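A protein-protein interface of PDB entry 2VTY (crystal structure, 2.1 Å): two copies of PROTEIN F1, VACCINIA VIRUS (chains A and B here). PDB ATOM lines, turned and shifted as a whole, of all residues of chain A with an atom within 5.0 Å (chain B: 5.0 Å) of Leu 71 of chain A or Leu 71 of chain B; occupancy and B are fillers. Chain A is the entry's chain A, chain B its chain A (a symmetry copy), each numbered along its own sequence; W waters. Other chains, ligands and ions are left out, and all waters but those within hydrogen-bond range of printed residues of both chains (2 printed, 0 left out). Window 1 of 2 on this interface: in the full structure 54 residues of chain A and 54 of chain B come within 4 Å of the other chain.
Water W2 bridges the side-chain hydroxyl of Tyr 64 of chain A and the side-chain carboxylate of Asp 72 of chain B. Water W1 bridges the side-chain hydroxyl (OH) of Tyr 64 of chain B and the side-chain carboxylate (OD1) of Asp 72 of chain A.
Leu 71 of chain B touches four residues of chain A. Printed residues of chain A within 4 Å of Tyr 75 of chain B: Tyr 64. Of the printed residues of chain B, Lys 68 of chain A touches Leu 71. Printed residues of chain B within 4 Å of Tyr 64 of chain A: Leu 71 (3.7 Å) and Tyr 75 (3.5 Å). The nearest printed residue of chain A that does not touch Ser 67 of chain B is Leu 74 of chain A (6.8 Å).
Hydrophobic or aromatic side chains of chain B that line the printed part of chain A: Tyr 64, Leu 71 and Tyr 75. Of the 10 printed residues of chain A, 5 touch a printed residue of chain B. Printed residues of chain A that touch a printed residue of chain B: Tyr 64, Ser 67, Lys 68, Leu 71 and Tyr 75. Among the printed residues, no Asp or Glu carboxylate lies within 4 Å of a Lys or Arg side-chain nitrogen of the other chain.
Tyr 64 of chain A touches Leu 71 of chain B, and with the chains exchanged Leu 71 of chain A touches Tyr 64 of chain B. Tyr 64 of chain A touches Tyr 75 of chain B, and with the chains exchanged Tyr 75 of chain A touches Tyr 64 of chain B. Ser 67 of chain A touches Leu 71 of chain B, and with the chains exchanged Leu 71 of chain A touches Ser 67 of chain B. Lys 68 of chain A touches Leu 71 of chain B, and with the chains exchanged Leu 71 of chain A touches Lys 68 of chain B.
O of Leu 71 of chain B touches CE1 of Tyr 64 of chain A, 3.7 Å away. Tyr 64 of chain A touches Tyr 75 of chain B (OH to CB, 3.5 Å). O of Ser 67 of chain A touches CD2 of Leu 71 of chain B (3.5 Å). N of Lys 68 of chain A touches CD2 of Leu 71 of chain B (3.6 Å). O of Leu 71 of chain A touches CE1 of Tyr 64 of chain B, at 3.7 Å. Leu 71 of chain A touches Ser 67 of chain B (CD2 to O, 3.5 Å). N of Lys 68 of chain B touches CD2 of Leu 71 of chain A, at 3.6 Å. Leu 71 of chain A touches Leu 71 of chain B (CD2 to CD2, 3.7 Å). Tyr 75 of chain A touches Tyr 64 of chain B.
The side-chain amino group of Lys 68 of chain B is in salt-bridge range of the side-chain carboxylate of Asp 72 of chain B (3.95 Å). The side-chain amino group (NZ) of Lys 68 of chain A is in salt-bridge range of the side-chain carboxylate (OD2) of Asp 72 of chain A (3.95 Å).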
ATOM      1  N   TYR A  64     -14.482 -34.784  18.467  1.00  0.00           N
ATOM      2  CA  TYR A  64     -13.748 -33.645  17.970  1.00  0.00           C
ATOM      3  C   TYR A  64     -13.522 -33.776  16.468  1.00  0.00           C
ATOM      4  O   TYR A  64     -13.762 -32.833  15.752  1.00  0.00           O
ATOM      5  CB  TYR A  64     -12.382 -33.488  18.690  1.00  0.00           C
ATOM      6  CG  TYR A  64     -11.634 -32.312  18.156  1.00  0.00           C
ATOM      7  CD1 TYR A  64     -11.925 -31.022  18.631  1.00  0.00           C
ATOM      8  CD2 TYR A  64     -10.696 -32.454  17.112  1.00  0.00           C
ATOM      9  CE1 TYR A  64     -11.272 -29.896  18.117  1.00  0.00           C
ATOM     10  CE2 TYR A  64     -10.045 -31.345  16.585  1.00  0.00           C
ATOM     11  CZ  TYR A  64     -10.351 -30.061  17.115  1.00  0.00           C
ATOM     12  OH  TYR A  64      -9.742 -28.915  16.650  1.00  0.00           O
ATOM     13  N   SER A  67     -16.836 -33.155  14.659  1.00  0.00           N
ATOM     14  CA  SER A  67     -17.286 -31.767  14.808  1.00  0.00           C
ATOM     15  C   SER A  67     -16.426 -30.801  14.008  1.00  0.00           C
ATOM     16  O   SER A  67     -16.915 -29.867  13.390  1.00  0.00           O
ATOM     17  CB  SER A  67     -17.287 -31.371  16.287  1.00  0.00           C
ATOM     18  OG  SER A  67     -18.343 -32.060  16.942  1.00  0.00           O
ATOM     19  N   LYS A  68     -15.139 -31.055  14.003  1.00  0.00           N
ATOM     20  CA  LYS A  68     -14.218 -30.183  13.295  1.00  0.00           C
ATOM     21  C   LYS A  68     -14.331 -30.361  11.799  1.00  0.00           C
ATOM     22  O   LYS A  68     -14.303 -29.373  11.067  1.00  0.00           O
ATOM     23  CB  LYS A  68     -12.769 -30.429  13.705  1.00  0.00           C
ATOM     24  CG  LYS A  68     -11.903 -29.242  13.302  1.00  0.00           C
ATOM     25  CD  LYS A  68     -10.631 -29.639  12.667  1.00  0.00           C
ATOM     26  CE  LYS A  68      -9.926 -28.372  12.204  1.00  0.00           C
ATOM     27  NZ  LYS A  68      -8.560 -28.718  11.854  1.00  0.00           N
ATOM     28  N   GLN A  69     -14.457 -31.602  11.337  1.00  0.00           N
ATOM     29  CA  GLN A  69     -14.749 -31.826   9.913  1.00  0.00           C
ATOM     30  C   GLN A  69     -16.061 -31.170   9.483  1.00  0.00           C
ATOM     31  O   GLN A  69     -16.127 -30.536   8.416  1.00  0.00           O
ATOM     32  CB  GLN A  69     -14.784 -33.317   9.588  1.00  0.00           C
ATOM     33  CG  GLN A  69     -13.435 -34.015   9.708  1.00  0.00           C
ATOM     34  CD  GLN A  69     -12.554 -33.757   8.493  1.00  0.00           C
ATOM     35  OE1 GLN A  69     -13.053 -33.677   7.377  1.00  0.00           O
ATOM     36  NE2 GLN A  69     -11.261 -33.626   8.705  1.00  0.00           N
ATOM     37  N   ARG A  70     -17.097 -31.298  10.314  1.00  0.00           N
ATOM     38  CA  ARG A  70     -18.380 -30.709   9.974  1.00  0.00           C
ATOM     39  C   ARG A  70     -18.265 -29.184   9.866  1.00  0.00           C
ATOM     40  O   ARG A  70     -18.811 -28.598   8.945  1.00  0.00           O
ATOM     41  CB  ARG A  70     -19.468 -31.088  10.984  1.00  0.00           C
ATOM     42  CG  ARG A  70     -20.884 -30.930  10.442  1.00  0.00           C
ATOM     43  CD  ARG A  70     -21.410 -29.500  10.522  1.00  0.00           C
ATOM     44  NE  ARG A  70     -22.575 -29.330   9.654  1.00  0.00           N
ATOM     45  CZ  ARG A  70     -22.510 -29.219   8.332  1.00  0.00           C
ATOM     46  NH1 ARG A  70     -21.312 -29.230   7.716  1.00  0.00           N
ATOM     47  NH2 ARG A  70     -23.646 -29.106   7.644  1.00  0.00           N
ATOM     48  N   LEU A  71     -17.564 -28.551  10.805  1.00  0.00           N
ATOM     49  CA  LEU A  71     -17.445 -27.095  10.813  1.00  0.00           C
ATOM     50  C   LEU A  71     -16.601 -26.633   9.636  1.00  0.00           C
ATOM     51  O   LEU A  71     -16.940 -25.660   8.962  1.00  0.00           O
ATOM     52  CB  LEU A  71     -16.869 -26.606  12.138  1.00  0.00           C
ATOM     53  CG  LEU A  71     -17.386 -25.313  12.770  1.00  0.00           C
ATOM     54  CD1 LEU A  71     -18.882 -25.153  12.651  1.00  0.00           C
ATOM     55  CD2 LEU A  71     -17.058 -25.362  14.238  1.00  0.00           C
ATOM     56  N   ASP A  72     -15.509 -27.335   9.347  1.00  0.00           N
ATOM     57  CA  ASP A  72     -14.703 -26.946   8.177  1.00  0.00           C
ATOM     58  C   ASP A  72     -15.517 -27.057   6.894  1.00  0.00           C
ATOM     59  O   ASP A  72     -15.458 -26.175   6.026  1.00  0.00           O
ATOM     60  CB  ASP A  72     -13.466 -27.800   8.061  1.00  0.00           C
ATOM     61  CG  ASP A  72     -12.428 -27.488   9.142  1.00  0.00           C
ATOM     62  OD1 ASP A  72     -12.551 -26.487   9.907  1.00  0.00           O
ATOM     63  OD2 ASP A  72     -11.474 -28.281   9.221  1.00  0.00           O
ATOM     64  N   ASP A  73     -16.262 -28.145   6.765  1.00  0.00           N
ATOM     65  CA  ASP A  73     -17.157 -28.330   5.632  1.00  0.00           C
ATOM     66  C   ASP A  73     -18.269 -27.282   5.526  1.00  0.00           C
ATOM     67  O   ASP A  73     -18.649 -26.872   4.415  1.00  0.00           O
ATOM     68  CB  ASP A  73     -17.812 -29.713   5.682  1.00  0.00           C
ATOM     69  CG  ASP A  73     -18.550 -30.036   4.398  1.00  0.00           C
ATOM     70  OD1 ASP A  73     -17.874 -30.406   3.406  1.00  0.00           O
ATOM     71  OD2 ASP A  73     -19.794 -29.896   4.385  1.00  0.00           O
ATOM     72  N   LEU A  74     -18.817 -26.869   6.666  1.00  0.00           N
ATOM     73  CA  LEU A  74     -19.881 -25.885   6.647  1.00  0.00           C
ATOM     74  C   LEU A  74     -19.331 -24.574   6.064  1.00  0.00           C
ATOM     75  O   LEU A  74     -19.931 -23.992   5.179  1.00  0.00           O
ATOM     76  CB  LEU A  74     -20.434 -25.653   8.053  1.00  0.00           C
ATOM     77  CG  LEU A  74     -21.468 -24.542   8.262  1.00  0.00           C
ATOM     78  CD1 LEU A  74     -22.678 -24.758   7.403  1.00  0.00           C
ATOM     79  CD2 LEU A  74     -21.853 -24.512   9.732  1.00  0.00           C
ATOM     80  N   TYR A  75     -18.173 -24.134   6.552  1.00  0.00           N
ATOM     81  CA  TYR A  75     -17.635 -22.904   6.090  1.00  0.00           C
ATOM     82  C   TYR A  75     -17.410 -22.979   4.582  1.00  0.00           C
ATOM     83  O   TYR A  75     -17.712 -22.023   3.851  1.00  0.00           O
ATOM     84  CB  TYR A  75     -16.341 -22.559   6.841  1.00  0.00           C
ATOM     85  CG  TYR A  75     -15.836 -21.185   6.458  1.00  0.00           C
ATOM     86  CD1 TYR A  75     -16.347 -20.037   7.104  1.00  0.00           C
ATOM     87  CD2 TYR A  75     -14.877 -21.022   5.432  1.00  0.00           C
ATOM     88  CE1 TYR A  75     -15.926 -18.767   6.753  1.00  0.00           C
ATOM     89  CE2 TYR A  75     -14.424 -19.732   5.044  1.00  0.00           C
ATOM     90  CZ  TYR A  75     -14.957 -18.609   5.724  1.00  0.00           C
ATOM     91  OH  TYR A  75     -14.552 -17.325   5.456  1.00  0.00           O
ATOM     92  N   TYR B  64     -21.831 -19.988  13.589  1.00  0.00           N
ATOM     93  CA  TYR B  64     -20.537 -20.434  13.133  1.00  0.00           C
ATOM     94  C   TYR B  64     -19.436 -19.850  14.011  1.00  0.00           C
ATOM     95  O   TYR B  64     -18.570 -20.579  14.432  1.00  0.00           O
ATOM     96  CB  TYR B  64     -20.286 -20.039  11.653  1.00  0.00           C
ATOM     97  CG  TYR B  64     -18.940 -20.499  11.202  1.00  0.00           C
ATOM     98  CD1 TYR B  64     -18.759 -21.827  10.779  1.00  0.00           C
ATOM     99  CD2 TYR B  64     -17.815 -19.652  11.276  1.00  0.00           C
ATOM    100  CE1 TYR B  64     -17.499 -22.299  10.393  1.00  0.00           C
ATOM    101  CE2 TYR B  64     -16.555 -20.108  10.905  1.00  0.00           C
ATOM    102  CZ  TYR B  64     -16.424 -21.452  10.456  1.00  0.00           C
ATOM    103  OH  TYR B  64     -15.210 -21.976  10.065  1.00  0.00           O
ATOM    104  N   SER B  67     -19.488 -21.621  17.402  1.00  0.00           N
ATOM    105  CA  SER B  67     -19.106 -23.033  17.285  1.00  0.00           C
ATOM    106  C   SER B  67     -17.625 -23.198  16.985  1.00  0.00           C
ATOM    107  O   SER B  67     -16.955 -24.071  17.518  1.00  0.00           O
ATOM    108  CB  SER B  67     -19.944 -23.714  16.201  1.00  0.00           C
ATOM    109  OG  SER B  67     -21.279 -23.843  16.670  1.00  0.00           O
ATOM    110  N   LYS B  68     -17.114 -22.330  16.145  1.00  0.00           N
ATOM    111  CA  LYS B  68     -15.715 -22.409  15.761  1.00  0.00           C
ATOM    112  C   LYS B  68     -14.810 -21.960  16.885  1.00  0.00           C
ATOM    113  O   LYS B  68     -13.777 -22.586  17.119  1.00  0.00           O
ATOM    114  CB  LYS B  68     -15.411 -21.565  14.528  1.00  0.00           C
ATOM    115  CG  LYS B  68     -14.093 -22.005  13.903  1.00  0.00           C
ATOM    116  CD  LYS B  68     -13.220 -20.875  13.530  1.00  0.00           C
ATOM    117  CE  LYS B  68     -11.898 -21.449  13.040  1.00  0.00           C
ATOM    118  NZ  LYS B  68     -11.153 -20.381  12.398  1.00  0.00           N
ATOM    119  N   GLN B  69     -15.182 -20.889  17.581  1.00  0.00           N
ATOM    120  CA  GLN B  69     -14.440 -20.511  18.793  1.00  0.00           C
ATOM    121  C   GLN B  69     -14.452 -21.620  19.847  1.00  0.00           C
ATOM    122  O   GLN B  69     -13.411 -21.921  20.455  1.00  0.00           O
ATOM    123  CB  GLN B  69     -14.991 -19.221  19.394  1.00  0.00           C
ATOM    124  CG  GLN B  69     -14.763 -17.985  18.533  1.00  0.00           C
ATOM    125  CD  GLN B  69     -13.341 -17.455  18.665  1.00  0.00           C
ATOM    126  OE1 GLN B  69     -12.764 -17.508  19.744  1.00  0.00           O
ATOM    127  NE2 GLN B  69     -12.783 -16.954  17.583  1.00  0.00           N
ATOM    128  N   ARG B  70     -15.614 -22.244  20.049  1.00  0.00           N
ATOM    129  CA  ARG B  70     -15.709 -23.304  21.037  1.00  0.00           C
ATOM    130  C   ARG B  70     -14.797 -24.478  20.662  1.00  0.00           C
ATOM    131  O   ARG B  70     -14.121 -25.019  21.522  1.00  0.00           O
ATOM    132  CB  ARG B  70     -17.151 -23.788  21.216  1.00  0.00           C
ATOM    133  CG  ARG B  70     -17.390 -24.512  22.537  1.00  0.00           C
ATOM    134  CD  ARG B  70     -16.976 -25.981  22.509  1.00  0.00           C
ATOM    135  NE  ARG B  70     -16.856 -26.507  23.868  1.00  0.00           N
ATOM    136  CZ  ARG B  70     -15.838 -26.248  24.681  1.00  0.00           C
ATOM    137  NH1 ARG B  70     -14.817 -25.480  24.255  1.00  0.00           N
ATOM    138  NH2 ARG B  70     -15.859 -26.757  25.914  1.00  0.00           N
ATOM    139  N   LEU B  71     -14.787 -24.868  19.389  1.00  0.00           N
ATOM    140  CA  LEU B  71     -13.990 -26.010  18.950  1.00  0.00           C
ATOM    141  C   LEU B  71     -12.509 -25.678  19.034  1.00  0.00           C
ATOM    142  O   LEU B  71     -11.706 -26.492  19.489  1.00  0.00           O
ATOM    143  CB  LEU B  71     -14.386 -26.438  17.540  1.00  0.00           C
ATOM    144  CG  LEU B  71     -14.426 -27.921  17.170  1.00  0.00           C
ATOM    145  CD1 LEU B  71     -15.001 -28.789  18.263  1.00  0.00           C
ATOM    146  CD2 LEU B  71     -15.321 -28.066  15.969  1.00  0.00           C
ATOM    147  N   ASP B  72     -12.124 -24.471  18.628  1.00  0.00           N
ATOM    148  CA  ASP B  72     -10.704 -24.099  18.752  1.00  0.00           C
ATOM    149  C   ASP B  72     -10.262 -24.116  20.209  1.00  0.00           C
ATOM    150  O   ASP B  72      -9.171 -24.605  20.537  1.00  0.00           O
ATOM    151  CB  ASP B  72     -10.446 -22.735  18.165  1.00  0.00           C
ATOM    152  CG  ASP B  72     -10.533 -22.722  16.637  1.00  0.00           C
ATOM    153  OD1 ASP B  72     -10.620 -23.795  15.971  1.00  0.00           O
ATOM    154  OD2 ASP B  72     -10.522 -21.599  16.103  1.00  0.00           O
ATOM    155  N   ASP B  73     -11.096 -23.567  21.080  1.00  0.00           N
ATOM    156  CA  ASP B  73     -10.837 -23.599  22.513  1.00  0.00           C
ATOM    157  C   ASP B  73     -10.777 -25.007  23.114  1.00  0.00           C
ATOM    158  O   ASP B  73      -9.975 -25.273  24.026  1.00  0.00           O
ATOM    159  CB  ASP B  73     -11.902 -22.804  23.272  1.00  0.00           C
ATOM    160  CG  ASP B  73     -11.530 -22.606  24.728  1.00  0.00           C
ATOM    161  OD1 ASP B  73     -10.687 -21.717  25.006  1.00  0.00           O
ATOM    162  OD2 ASP B  73     -12.065 -23.354  25.577  1.00  0.00           O
ATOM    163  N   LEU B  74     -11.639 -25.902  22.637  1.00  0.00           N
ATOM    164  CA  LEU B  74     -11.649 -27.253  23.161  1.00  0.00           C
ATOM    165  C   LEU B  74     -10.297 -27.914  22.850  1.00  0.00           C
ATOM    166  O   LEU B  74      -9.675 -28.488  23.724  1.00  0.00           O
ATOM    167  CB  LEU B  74     -12.793 -28.064  22.552  1.00  0.00           C
ATOM    168  CG  LEU B  74     -12.884 -29.560  22.872  1.00  0.00           C
ATOM    169  CD1 LEU B  74     -12.990 -29.794  24.350  1.00  0.00           C
ATOM    170  CD2 LEU B  74     -14.093 -30.135  22.151  1.00  0.00           C
ATOM    171  N   TYR B  75      -9.843 -27.803  21.603  1.00  0.00           N
ATOM    172  CA  TYR B  75      -8.623 -28.432  21.239  1.00  0.00           C
ATOM    173  C   TYR B  75      -7.491 -27.894  22.108  1.00  0.00           C
ATOM    174  O   TYR B  75      -6.637 -28.661  22.580  1.00  0.00           O
ATOM    175  CB  TYR B  75      -8.334 -28.237  19.744  1.00  0.00           C
ATOM    176  CG  TYR B  75      -7.113 -29.021  19.315  1.00  0.00           C
ATOM    177  CD1 TYR B  75      -7.234 -30.384  18.966  1.00  0.00           C
ATOM    178  CD2 TYR B  75      -5.834 -28.419  19.288  1.00  0.00           C
ATOM    179  CE1 TYR B  75      -6.130 -31.133  18.600  1.00  0.00           C
ATOM    180  CE2 TYR B  75      -4.679 -29.159  18.921  1.00  0.00           C
ATOM    181  CZ  TYR B  75      -4.846 -30.521  18.570  1.00  0.00           C
ATOM    182  OH  TYR B  75      -3.802 -31.310  18.157  1.00  0.00           O
HETATM  183  O   HOH W   1     -13.584 -23.887   9.522  1.00  0.00           O
HETATM  184  O   HOH W   2      -9.532 -26.376  16.330  1.00  0.00           O
